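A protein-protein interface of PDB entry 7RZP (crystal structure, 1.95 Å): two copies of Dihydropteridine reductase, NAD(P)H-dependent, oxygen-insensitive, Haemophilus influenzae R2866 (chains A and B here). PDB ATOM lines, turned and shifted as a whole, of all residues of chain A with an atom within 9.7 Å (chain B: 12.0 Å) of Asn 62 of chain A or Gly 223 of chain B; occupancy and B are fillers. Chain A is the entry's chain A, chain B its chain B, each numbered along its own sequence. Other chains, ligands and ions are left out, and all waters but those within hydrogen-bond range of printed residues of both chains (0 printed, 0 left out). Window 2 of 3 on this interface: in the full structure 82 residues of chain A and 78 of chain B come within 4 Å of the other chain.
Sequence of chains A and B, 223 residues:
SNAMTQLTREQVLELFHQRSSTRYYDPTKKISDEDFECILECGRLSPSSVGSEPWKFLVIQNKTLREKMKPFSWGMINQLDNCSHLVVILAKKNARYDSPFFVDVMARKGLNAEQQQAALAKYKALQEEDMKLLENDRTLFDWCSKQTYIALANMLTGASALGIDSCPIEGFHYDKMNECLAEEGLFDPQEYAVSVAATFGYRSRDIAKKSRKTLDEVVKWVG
N of Val 59 of chain A sits at hydrogen-bond distance from O of Lys 220 of chain B (2.9 Å). O of Val 59 of chain A sits at hydrogen-bond distance from N of Val 222 of chain B, 2.8 Å away. The backbone carbonyl oxygen (O) of Val 222 of chain B lies within hydrogen-bond range of the backbone NH (N) of Gln 61 of chain A, 3.0 Å away. The backbone NH (N) of Asn 62 of chain A is in hydrogen-bond range of the backbone carbonyl oxygen (O) of Val 222 of chain B (3.0 Å). The chain-end carboxylate of Gly 223 of chain B lies within hydrogen-bond range of the side-chain amide nitrogen of Asn 62 of chain A, 3.0 Å away.
The backbone carbonyl oxygen (O) of Ile 60 of chain A sits at hydrogen-bond distance from the guanidinium group (NE) of Arg 66 of chain A (2.8 Å). The side-chain amide oxygen (OE1) of Gln 61 of chain A is in hydrogen-bond range of the backbone NH (N) of Leu 86 of chain A (3.2 Å). The backbone NH (N) of Thr 64 of chain A lies within hydrogen-bond range of the side-chain amide oxygen (OD1) of Asn 62 of chain A (3.1 Å). The side-chain amide oxygen (OD1) of Asn 62 of chain A is in hydrogen-bond range of the backbone NH (N) of Leu 65 of chain A (2.8 Å). The side-chain hydroxyl (OG) of Ser 84 of chain A lies within hydrogen-bond range of a ring nitrogen (ND1) of His 85 of chain A, 2.8 Å away. The backbone carbonyl oxygen (O) of Leu 181 of chain A is in hydrogen-bond range of the backbone NH (N) of Leu 186 of chain A.
Among the printed residues, merely in contact across the chains: Leu 58 of chain A with Lys 220 of chain B, Val 59 of chain A with Val 219 of chain B, Val 59 of chain A with Trp 221 of chain B, Ile 60 of chain A with Val 222 of chain B, Gln 61 of chain A with Trp 221 of chain B, His 85 of chain A with Trp 221 of chain B, Leu 186 of chain A with Lys 220 of chain B and Leu 186 of chain A with Val 222 of chain B.
Of chain B, only Val 222 (3.9 Å) comes within 4 Å of Ile 60 of chain A. Gln 61 of chain A touches two residues of chain B. Asn 62 of chain A touches just these residues of chain B: Val 222 (3.0 Å) and Gly 223 (3.0 Å). No residue of chain B comes within 4 Å of Lys 63 of chain A. No residue of chain B comes within 4 Å of Thr 64 of chain A. Of the printed residues of chain A, Lys 220 of chain B touches Leu 58, Val 59 and Leu 186. Of the printed residues of chain A, Trp 221 of chain B touches Val 59 (3.8 Å), Gln 61 (3.7 Å) and His 85 (3.7 Å). Val 222 of chain B touches just these residues of chain A: Val 59 (2.8 Å), Ile 60 (3.9 Å), Gln 61 (3.0 Å), Asn 62 (3.0 Å) and Leu 186 (3.9 Å). Gly 223 of chain B touches just one residue of chain A: Asn 62 (3.0 Å). The nearest residue of chain B that does not touch Asn 62 of chain A is Trp 221 of chain B (6.7 Å).
Printed residues of chain A that touch a printed residue of chain B: Leu 58, Val 59, Ile 60, Gln 61, Asn 62, His 85 and Leu 186. Along chain A the printed residues that touch a printed residue of chain B span positions 58 to 186. Among the printed residues, 13 pairs touch across the chains. Among the printed residues, no Asp or Glu carboxylate lies within 4 Å of a Lys or Arg side-chain nitrogen of the other chain.
No position is printed for both chains. Of the 13 pairs that touch across the chains among the printed residues, none has its exchanged pair printed and touching as well.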
ATOM      1  N   LEU A  58       5.124  -6.056  -9.370  1.00  0.00           N
ATOM      2  CA  LEU A  58       4.364  -7.134  -8.747  1.00  0.00           C
ATOM      3  C   LEU A  58       5.107  -8.451  -8.952  1.00  0.00           C
ATOM      4  O   LEU A  58       5.456  -8.785 -10.079  1.00  0.00           O
ATOM      5  CB  LEU A  58       2.981  -7.228  -9.374  1.00  0.00           C
ATOM      6  CG  LEU A  58       2.207  -5.912  -9.464  1.00  0.00           C
ATOM      7  CD1 LEU A  58       0.785  -6.192  -9.985  1.00  0.00           C
ATOM      8  CD2 LEU A  58       2.172  -5.154  -8.141  1.00  0.00           C
ATOM      9  N   VAL A  59       5.354  -9.201  -7.877  1.00  0.00           N
ATOM     10  CA  VAL A  59       6.002 -10.514  -7.957  1.00  0.00           C
ATOM     11  C   VAL A  59       4.919 -11.570  -7.717  1.00  0.00           C
ATOM     12  O   VAL A  59       4.482 -11.759  -6.572  1.00  0.00           O
ATOM     13  CB  VAL A  59       7.161 -10.652  -6.951  1.00  0.00           C
ATOM     14  CG1 VAL A  59       7.862 -11.972  -7.106  1.00  0.00           C
ATOM     15  CG2 VAL A  59       8.202  -9.521  -7.137  1.00  0.00           C
ATOM     16  N   ILE A  60       4.486 -12.258  -8.783  1.00  0.00           N
ATOM     17  CA  ILE A  60       3.304 -13.133  -8.742  1.00  0.00           C
ATOM     18  C   ILE A  60       3.777 -14.569  -8.524  1.00  0.00           C
ATOM     19  O   ILE A  60       3.984 -15.336  -9.480  1.00  0.00           O
ATOM     20  CB  ILE A  60       2.458 -13.019 -10.006  1.00  0.00           C
ATOM     21  CG1 ILE A  60       2.262 -11.551 -10.421  1.00  0.00           C
ATOM     22  CG2 ILE A  60       1.128 -13.774  -9.821  1.00  0.00           C
ATOM     23  CD1 ILE A  60       1.326 -10.811  -9.581  1.00  0.00           C
ATOM     24  N   GLN A  61       3.899 -14.954  -7.244  1.00  0.00           N
ATOM     25  CA  GLN A  61       4.269 -16.309  -6.835  1.00  0.00           C
ATOM     26  C   GLN A  61       3.063 -17.179  -6.481  1.00  0.00           C
ATOM     27  O   GLN A  61       3.160 -18.418  -6.516  1.00  0.00           O
ATOM     28  CB  GLN A  61       5.223 -16.232  -5.640  1.00  0.00           C
ATOM     29  CG  GLN A  61       6.514 -15.482  -5.957  1.00  0.00           C
ATOM     30  CD  GLN A  61       7.315 -16.115  -7.110  1.00  0.00           C
ATOM     31  OE1 GLN A  61       7.178 -15.743  -8.290  1.00  0.00           O
ATOM     32  NE2 GLN A  61       8.185 -17.054  -6.753  1.00  0.00           N
ATOM     33  N   ASN A  62       1.926 -16.571  -6.185  1.00  0.00           N
ATOM     34  CA  ASN A  62       0.705 -17.335  -5.923  1.00  0.00           C
ATOM     35  C   ASN A  62       0.348 -18.238  -7.097  1.00  0.00           C
ATOM     36  O   ASN A  62       0.073 -17.753  -8.201  1.00  0.00           O
ATOM     37  CB  ASN A  62      -0.450 -16.388  -5.656  1.00  0.00           C
ATOM     38  CG  ASN A  62      -1.652 -17.097  -5.135  1.00  0.00           C
ATOM     39  OD1 ASN A  62      -2.521 -17.494  -5.898  1.00  0.00           O
ATOM     40  ND2 ASN A  62      -1.734 -17.241  -3.816  1.00  0.00           N
ATOM     41  N   LYS A  63       0.295 -19.549  -6.837  1.00  0.00           N
ATOM     42  CA  LYS A  63       0.013 -20.511  -7.903  1.00  0.00           C
ATOM     43  C   LYS A  63      -1.401 -20.369  -8.444  1.00  0.00           C
ATOM     44  O   LYS A  63      -1.618 -20.515  -9.648  1.00  0.00           O
ATOM     45  CB  LYS A  63       0.282 -21.930  -7.402  1.00  0.00           C
ATOM     46  CG  LYS A  63       1.730 -22.082  -6.933  1.00  0.00           C
ATOM     47  CD  LYS A  63       2.367 -23.418  -7.390  1.00  0.00           C
ATOM     48  CE  LYS A  63       3.874 -23.437  -7.077  1.00  0.00           C
ATOM     49  NZ  LYS A  63       4.308 -22.070  -6.583  1.00  0.00           N
ATOM     50  N   THR A  64      -2.370 -20.056  -7.589  1.00  0.00           N
ATOM     51  CA  THR A  64      -3.738 -19.891  -8.068  1.00  0.00           C
ATOM     52  C   THR A  64      -3.883 -18.659  -8.963  1.00  0.00           C
ATOM     53  O   THR A  64      -4.608 -18.700  -9.966  1.00  0.00           O
ATOM     54  CB  THR A  64      -4.690 -19.818  -6.880  1.00  0.00           C
ATOM     55  OG1 THR A  64      -4.677 -21.080  -6.209  1.00  0.00           O
ATOM     56  CG2 THR A  64      -6.103 -19.512  -7.345  1.00  0.00           C
ATOM     57  N   LEU A  65      -3.212 -17.552  -8.622  1.00  0.00           N
ATOM     58  CA  LEU A  65      -3.282 -16.380  -9.485  1.00  0.00           C
ATOM     59  C   LEU A  65      -2.630 -16.658 -10.822  1.00  0.00           C
ATOM     60  O   LEU A  65      -3.176 -16.297 -11.869  1.00  0.00           O
ATOM     61  CB  LEU A  65      -2.617 -15.170  -8.824  1.00  0.00           C
ATOM     62  CG  LEU A  65      -2.744 -13.865  -9.626  1.00  0.00           C
ATOM     63  CD1 LEU A  65      -4.182 -13.563  -9.978  1.00  0.00           C
ATOM     64  CD2 LEU A  65      -2.174 -12.706  -8.820  1.00  0.00           C
ATOM     65  N   ARG A  66      -1.463 -17.302 -10.804  1.00  0.00           N
ATOM     66  CA  ARG A  66      -0.807 -17.701 -12.042  1.00  0.00           C
ATOM     67  C   ARG A  66      -1.754 -18.502 -12.943  1.00  0.00           C
ATOM     68  O   ARG A  66      -1.848 -18.247 -14.151  1.00  0.00           O
ATOM     69  CB  ARG A  66       0.448 -18.510 -11.704  1.00  0.00           C
ATOM     70  CG  ARG A  66       1.634 -17.677 -11.200  1.00  0.00           C
ATOM     71  CD  ARG A  66       2.920 -18.496 -11.315  1.00  0.00           C
ATOM     72  NE  ARG A  66       4.072 -17.860 -10.688  1.00  0.00           N
ATOM     73  CZ  ARG A  66       5.266 -18.432 -10.586  1.00  0.00           C
ATOM     74  NH1 ARG A  66       5.483 -19.647 -11.055  1.00  0.00           N
ATOM     75  NH2 ARG A  66       6.273 -17.755 -10.029  1.00  0.00           N
ATOM     76  N   GLU A  67      -2.469 -19.481 -12.368  1.00  0.00           N
ATOM     77  CA  GLU A  67      -3.405 -20.296 -13.146  1.00  0.00           C
ATOM     78  C   GLU A  67      -4.476 -19.431 -13.795  1.00  0.00           C
ATOM     79  O   GLU A  67      -4.846 -19.638 -14.958  1.00  0.00           O
ATOM     80  CB  GLU A  67      -4.056 -21.345 -12.232  1.00  0.00           C
ATOM     81  CG  GLU A  67      -4.719 -22.581 -12.866  1.00  0.00           C
ATOM     82  CD  GLU A  67      -3.739 -23.545 -13.538  1.00  0.00           C
ATOM     83  OE1 GLU A  67      -2.817 -24.046 -12.840  1.00  0.00           O
ATOM     84  OE2 GLU A  67      -3.940 -23.871 -14.737  1.00  0.00           O
ATOM     85  N   LYS A  68      -4.982 -18.455 -13.050  1.00  0.00           N
ATOM     86  CA  LYS A  68      -6.081 -17.628 -13.510  1.00  0.00           C
ATOM     87  C   LYS A  68      -5.683 -16.770 -14.704  1.00  0.00           C
ATOM     88  O   LYS A  68      -6.562 -16.352 -15.469  1.00  0.00           O
ATOM     89  CB  LYS A  68      -6.555 -16.770 -12.329  1.00  0.00           C
ATOM     90  CG  LYS A  68      -7.563 -15.653 -12.627  1.00  0.00           C
ATOM     91  CD  LYS A  68      -7.941 -14.901 -11.317  1.00  0.00           C
ATOM     92  CE  LYS A  68      -8.873 -13.718 -11.569  1.00  0.00           C
ATOM     93  NZ  LYS A  68     -10.200 -14.251 -12.017  1.00  0.00           N
ATOM     94  N   MET A  69      -4.386 -16.530 -14.898  1.00  0.00           N
ATOM     95  CA  MET A  69      -3.903 -15.699 -15.996  1.00  0.00           C
ATOM     96  C   MET A  69      -3.744 -16.450 -17.309  1.00  0.00           C
ATOM     97  O   MET A  69      -3.747 -15.841 -18.390  1.00  0.00           O
ATOM     98  CB  MET A  69      -2.546 -15.066 -15.669  1.00  0.00           C
ATOM     99  CG  MET A  69      -2.490 -14.142 -14.466  1.00  0.00           C
ATOM    100  SD  MET A  69      -0.603 -13.814 -14.045  1.00  0.00           S
ATOM    101  CE  MET A  69      -0.716 -12.048 -13.252  1.00  0.00           C
ATOM    102  N   LYS A  70      -3.580 -17.769 -17.209  1.00  0.00           N
ATOM    103  CA  LYS A  70      -3.331 -18.598 -18.389  1.00  0.00           C
ATOM    104  C   LYS A  70      -4.305 -18.361 -19.536  1.00  0.00           C
ATOM    105  O   LYS A  70      -3.841 -18.233 -20.677  1.00  0.00           O
ATOM    106  CB  LYS A  70      -3.322 -20.077 -17.978  1.00  0.00           C
ATOM    107  CG  LYS A  70      -2.287 -20.377 -16.924  1.00  0.00           C
ATOM    108  CD  LYS A  70      -1.426 -21.560 -17.291  1.00  0.00           C
ATOM    109  CE  LYS A  70      -2.137 -22.829 -16.987  1.00  0.00           C
ATOM    110  NZ  LYS A  70      -1.200 -23.776 -16.343  1.00  0.00           N
ATOM    111  N   LEU A  80       3.997 -20.148 -17.165  1.00  0.00           N
ATOM    112  CA  LEU A  80       3.387 -19.828 -15.878  1.00  0.00           C
ATOM    113  C   LEU A  80       3.493 -20.992 -14.907  1.00  0.00           C
ATOM    114  O   LEU A  80       3.688 -20.770 -13.706  1.00  0.00           O
ATOM    115  CB  LEU A  80       1.928 -19.430 -16.066  1.00  0.00           C
ATOM    116  CG  LEU A  80       1.796 -18.004 -16.581  1.00  0.00           C
ATOM    117  CD1 LEU A  80       0.419 -17.766 -17.165  1.00  0.00           C
ATOM    118  CD2 LEU A  80       2.112 -17.017 -15.452  1.00  0.00           C
ATOM    119  N   ASP A  81       3.417 -22.232 -15.409  1.00  0.00           N
ATOM    120  CA  ASP A  81       3.485 -23.410 -14.542  1.00  0.00           C
ATOM    121  C   ASP A  81       4.881 -23.612 -13.946  1.00  0.00           C
ATOM    122  O   ASP A  81       5.012 -24.014 -12.782  1.00  0.00           O
ATOM    123  CB  ASP A  81       3.077 -24.672 -15.309  1.00  0.00           C
ATOM    124  CG  ASP A  81       1.588 -24.722 -15.630  1.00  0.00           C
ATOM    125  OD1 ASP A  81       0.773 -24.542 -14.691  1.00  0.00           O
ATOM    126  OD2 ASP A  81       1.238 -25.013 -16.805  1.00  0.00           O
ATOM    127  N   CYS A  83       8.094 -21.556 -14.406  1.00  0.00           N
ATOM    128  CA  CYS A  83       9.056 -20.535 -14.032  1.00  0.00           C
ATOM    129  C   CYS A  83       9.181 -20.437 -12.514  1.00  0.00           C
ATOM    130  O   CYS A  83       8.281 -20.822 -11.759  1.00  0.00           O
ATOM    131  CB  CYS A  83       8.677 -19.187 -14.652  1.00  0.00           C
ATOM    132  SG  CYS A  83       7.221 -18.340 -14.009  1.00  0.00           S
ATOM    133  N   SER A  84      10.352 -19.970 -12.073  1.00  0.00           N
ATOM    134  CA  SER A  84      10.582 -19.762 -10.651  1.00  0.00           C
ATOM    135  C   SER A  84       9.806 -18.557 -10.159  1.00  0.00           C
ATOM    136  O   SER A  84       9.091 -18.628  -9.150  1.00  0.00           O
ATOM    137  CB  SER A  84      12.072 -19.577 -10.387  1.00  0.00           C
ATOM    138  OG  SER A  84      12.301 -19.345  -9.006  1.00  0.00           O
ATOM    139  N   HIS A  85       9.915 -17.450 -10.883  1.00  0.00           N
ATOM    140  CA  HIS A  85       9.390 -16.170 -10.447  1.00  0.00           C
ATOM    141  C   HIS A  85       8.702 -15.474 -11.611  1.00  0.00           C
ATOM    142  O   HIS A  85       9.141 -15.599 -12.758  1.00  0.00           O
ATOM    143  CB  HIS A  85      10.523 -15.275  -9.914  1.00  0.00           C
ATOM    144  CG  HIS A  85      10.943 -15.588  -8.514  1.00  0.00           C
ATOM    145  ND1 HIS A  85      11.526 -16.786  -8.162  1.00  0.00           N
ATOM    146  CD2 HIS A  85      10.874 -14.854  -7.380  1.00  0.00           C
ATOM    147  CE1 HIS A  85      11.793 -16.783  -6.869  1.00  0.00           C
ATOM    148  NE2 HIS A  85      11.408 -15.621  -6.370  1.00  0.00           N
ATOM    149  N   LEU A  86       7.634 -14.730 -11.312  1.00  0.00           N
ATOM    150  CA  LEU A  86       6.948 -13.892 -12.300  1.00  0.00           C
ATOM    151  C   LEU A  86       6.848 -12.462 -11.775  1.00  0.00           C
ATOM    152  O   LEU A  86       6.326 -12.238 -10.670  1.00  0.00           O
ATOM    153  CB  LEU A  86       5.547 -14.427 -12.588  1.00  0.00           C
ATOM    154  CG  LEU A  86       4.646 -13.526 -13.441  1.00  0.00           C
ATOM    155  CD1 LEU A  86       5.213 -13.407 -14.858  1.00  0.00           C
ATOM    156  CD2 LEU A  86       3.212 -14.053 -13.454  1.00  0.00           C
ATOM    157  N   LEU A 181      -5.795  -8.267 -12.244  1.00  0.00           N
ATOM    158  CA  LEU A 181      -4.915  -7.879 -11.152  1.00  0.00           C
ATOM    159  C   LEU A 181      -5.546  -6.810 -10.268  1.00  0.00           C
ATOM    160  O   LEU A 181      -5.320  -6.790  -9.053  1.00  0.00           O
ATOM    161  CB  LEU A 181      -3.583  -7.387 -11.725  1.00  0.00           C
ATOM    162  CG  LEU A 181      -2.733  -8.437 -12.443  1.00  0.00           C
ATOM    163  CD1 LEU A 181      -1.339  -7.927 -12.849  1.00  0.00           C
ATOM    164  CD2 LEU A 181      -2.594  -9.598 -11.459  1.00  0.00           C
ATOM    165  N   GLU A 184      -8.125  -8.359  -8.109  1.00  0.00           N
ATOM    166  CA  GLU A 184      -7.443  -9.079  -7.043  1.00  0.00           C
ATOM    167  C   GLU A 184      -6.828  -8.149  -6.007  1.00  0.00           C
ATOM    168  O   GLU A 184      -6.124  -8.631  -5.111  1.00  0.00           O
ATOM    169  CB  GLU A 184      -6.332  -9.960  -7.614  1.00  0.00           C
ATOM    170  CG  GLU A 184      -6.843 -11.119  -8.411  1.00  0.00           C
ATOM    171  CD  GLU A 184      -7.446 -12.150  -7.533  1.00  0.00           C
ATOM    172  OE1 GLU A 184      -6.814 -12.472  -6.502  1.00  0.00           O
ATOM    173  OE2 GLU A 184      -8.555 -12.633  -7.867  1.00  0.00           O
ATOM    174  N   LEU A 186      -4.428  -5.761  -6.324  1.00  0.00           N
ATOM    175  CA  LEU A 186      -2.978  -5.644  -6.332  1.00  0.00           C
ATOM    176  C   LEU A 186      -2.485  -4.253  -6.705  1.00  0.00           C
ATOM    177  O   LEU A 186      -1.314  -3.947  -6.439  1.00  0.00           O
ATOM    178  CB  LEU A 186      -2.376  -6.690  -7.277  1.00  0.00           C
ATOM    179  CG  LEU A 186      -2.753  -8.158  -6.953  1.00  0.00           C
ATOM    180  CD1 LEU A 186      -1.903  -9.138  -7.763  1.00  0.00           C
ATOM    181  CD2 LEU A 186      -2.612  -8.483  -5.474  1.00  0.00           C
ATOM    182  N   VAL B 219       8.397  -2.866  -4.784  1.00  0.00           N
ATOM    183  CA  VAL B 219       8.072  -4.284  -4.959  1.00  0.00           C
ATOM    184  C   VAL B 219       6.798  -4.587  -4.171  1.00  0.00           C
ATOM    185  O   VAL B 219       6.641  -4.134  -3.032  1.00  0.00           O
ATOM    186  CB  VAL B 219       9.240  -5.188  -4.508  1.00  0.00           C
ATOM    187  CG1 VAL B 219       8.882  -6.669  -4.661  1.00  0.00           C
ATOM    188  CG2 VAL B 219      10.507  -4.865  -5.281  1.00  0.00           C
ATOM    189  N   LYS B 220       5.867  -5.309  -4.787  1.00  0.00           N
ATOM    190  CA  LYS B 220       4.747  -5.909  -4.064  1.00  0.00           C
ATOM    191  C   LYS B 220       4.819  -7.421  -4.253  1.00  0.00           C
ATOM    192  O   LYS B 220       4.645  -7.925  -5.373  1.00  0.00           O
ATOM    193  CB  LYS B 220       3.399  -5.373  -4.532  1.00  0.00           C
ATOM    194  CG  LYS B 220       2.234  -5.747  -3.620  1.00  0.00           C
ATOM    195  CD  LYS B 220       0.952  -5.123  -4.129  1.00  0.00           C
ATOM    196  CE  LYS B 220      -0.124  -5.148  -3.069  1.00  0.00           C
ATOM    197  NZ  LYS B 220       0.377  -4.786  -1.698  1.00  0.00           N
ATOM    198  N   TRP B 221       5.081  -8.142  -3.165  1.00  0.00           N
ATOM    199  CA  TRP B 221       5.186  -9.592  -3.224  1.00  0.00           C
ATOM    200  C   TRP B 221       3.790 -10.173  -3.080  1.00  0.00           C
ATOM    201  O   TRP B 221       3.089  -9.903  -2.094  1.00  0.00           O
ATOM    202  CB  TRP B 221       6.120 -10.133  -2.147  1.00  0.00           C
ATOM    203  CG  TRP B 221       6.677 -11.455  -2.494  1.00  0.00           C
ATOM    204  CD1 TRP B 221       6.090 -12.697  -2.295  1.00  0.00           C
ATOM    205  CD2 TRP B 221       7.957 -11.712  -3.096  1.00  0.00           C
ATOM    206  NE1 TRP B 221       6.937 -13.695  -2.744  1.00  0.00           N
ATOM    207  CE2 TRP B 221       8.080 -13.117  -3.244  1.00  0.00           C
ATOM    208  CE3 TRP B 221       9.011 -10.893  -3.516  1.00  0.00           C
ATOM    209  CZ2 TRP B 221       9.216 -13.709  -3.791  1.00  0.00           C
ATOM    210  CZ3 TRP B 221      10.139 -11.483  -4.065  1.00  0.00           C
ATOM    211  CH2 TRP B 221      10.229 -12.876  -4.204  1.00  0.00           C
ATOM    212  N   VAL B 222       3.398 -10.984  -4.062  1.00  0.00           N
ATOM    213  CA  VAL B 222       2.097 -11.643  -4.089  1.00  0.00           C
ATOM    214  C   VAL B 222       2.269 -13.153  -3.967  1.00  0.00           C
ATOM    215  O   VAL B 222       2.328 -13.872  -4.974  1.00  0.00           O
ATOM    216  CB  VAL B 222       1.324 -11.291  -5.370  1.00  0.00           C
ATOM    217  CG1 VAL B 222      -0.060 -11.899  -5.305  1.00  0.00           C
ATOM    218  CG2 VAL B 222       1.255  -9.765  -5.573  1.00  0.00           C
ATOM    219  N   GLY B 223       2.348 -13.643  -2.731  1.00  0.00           N
ATOM    220  CA  GLY B 223       2.703 -15.026  -2.480  1.00  0.00           C
ATOM    221  C   GLY B 223       1.508 -15.954  -2.525  1.00  0.00           C
ATOM    222  O   GLY B 223       1.684 -17.163  -2.592  1.00  0.00           O
ATOM    223  OXT GLY B 223       0.341 -15.533  -2.474  1.00  0.00           O
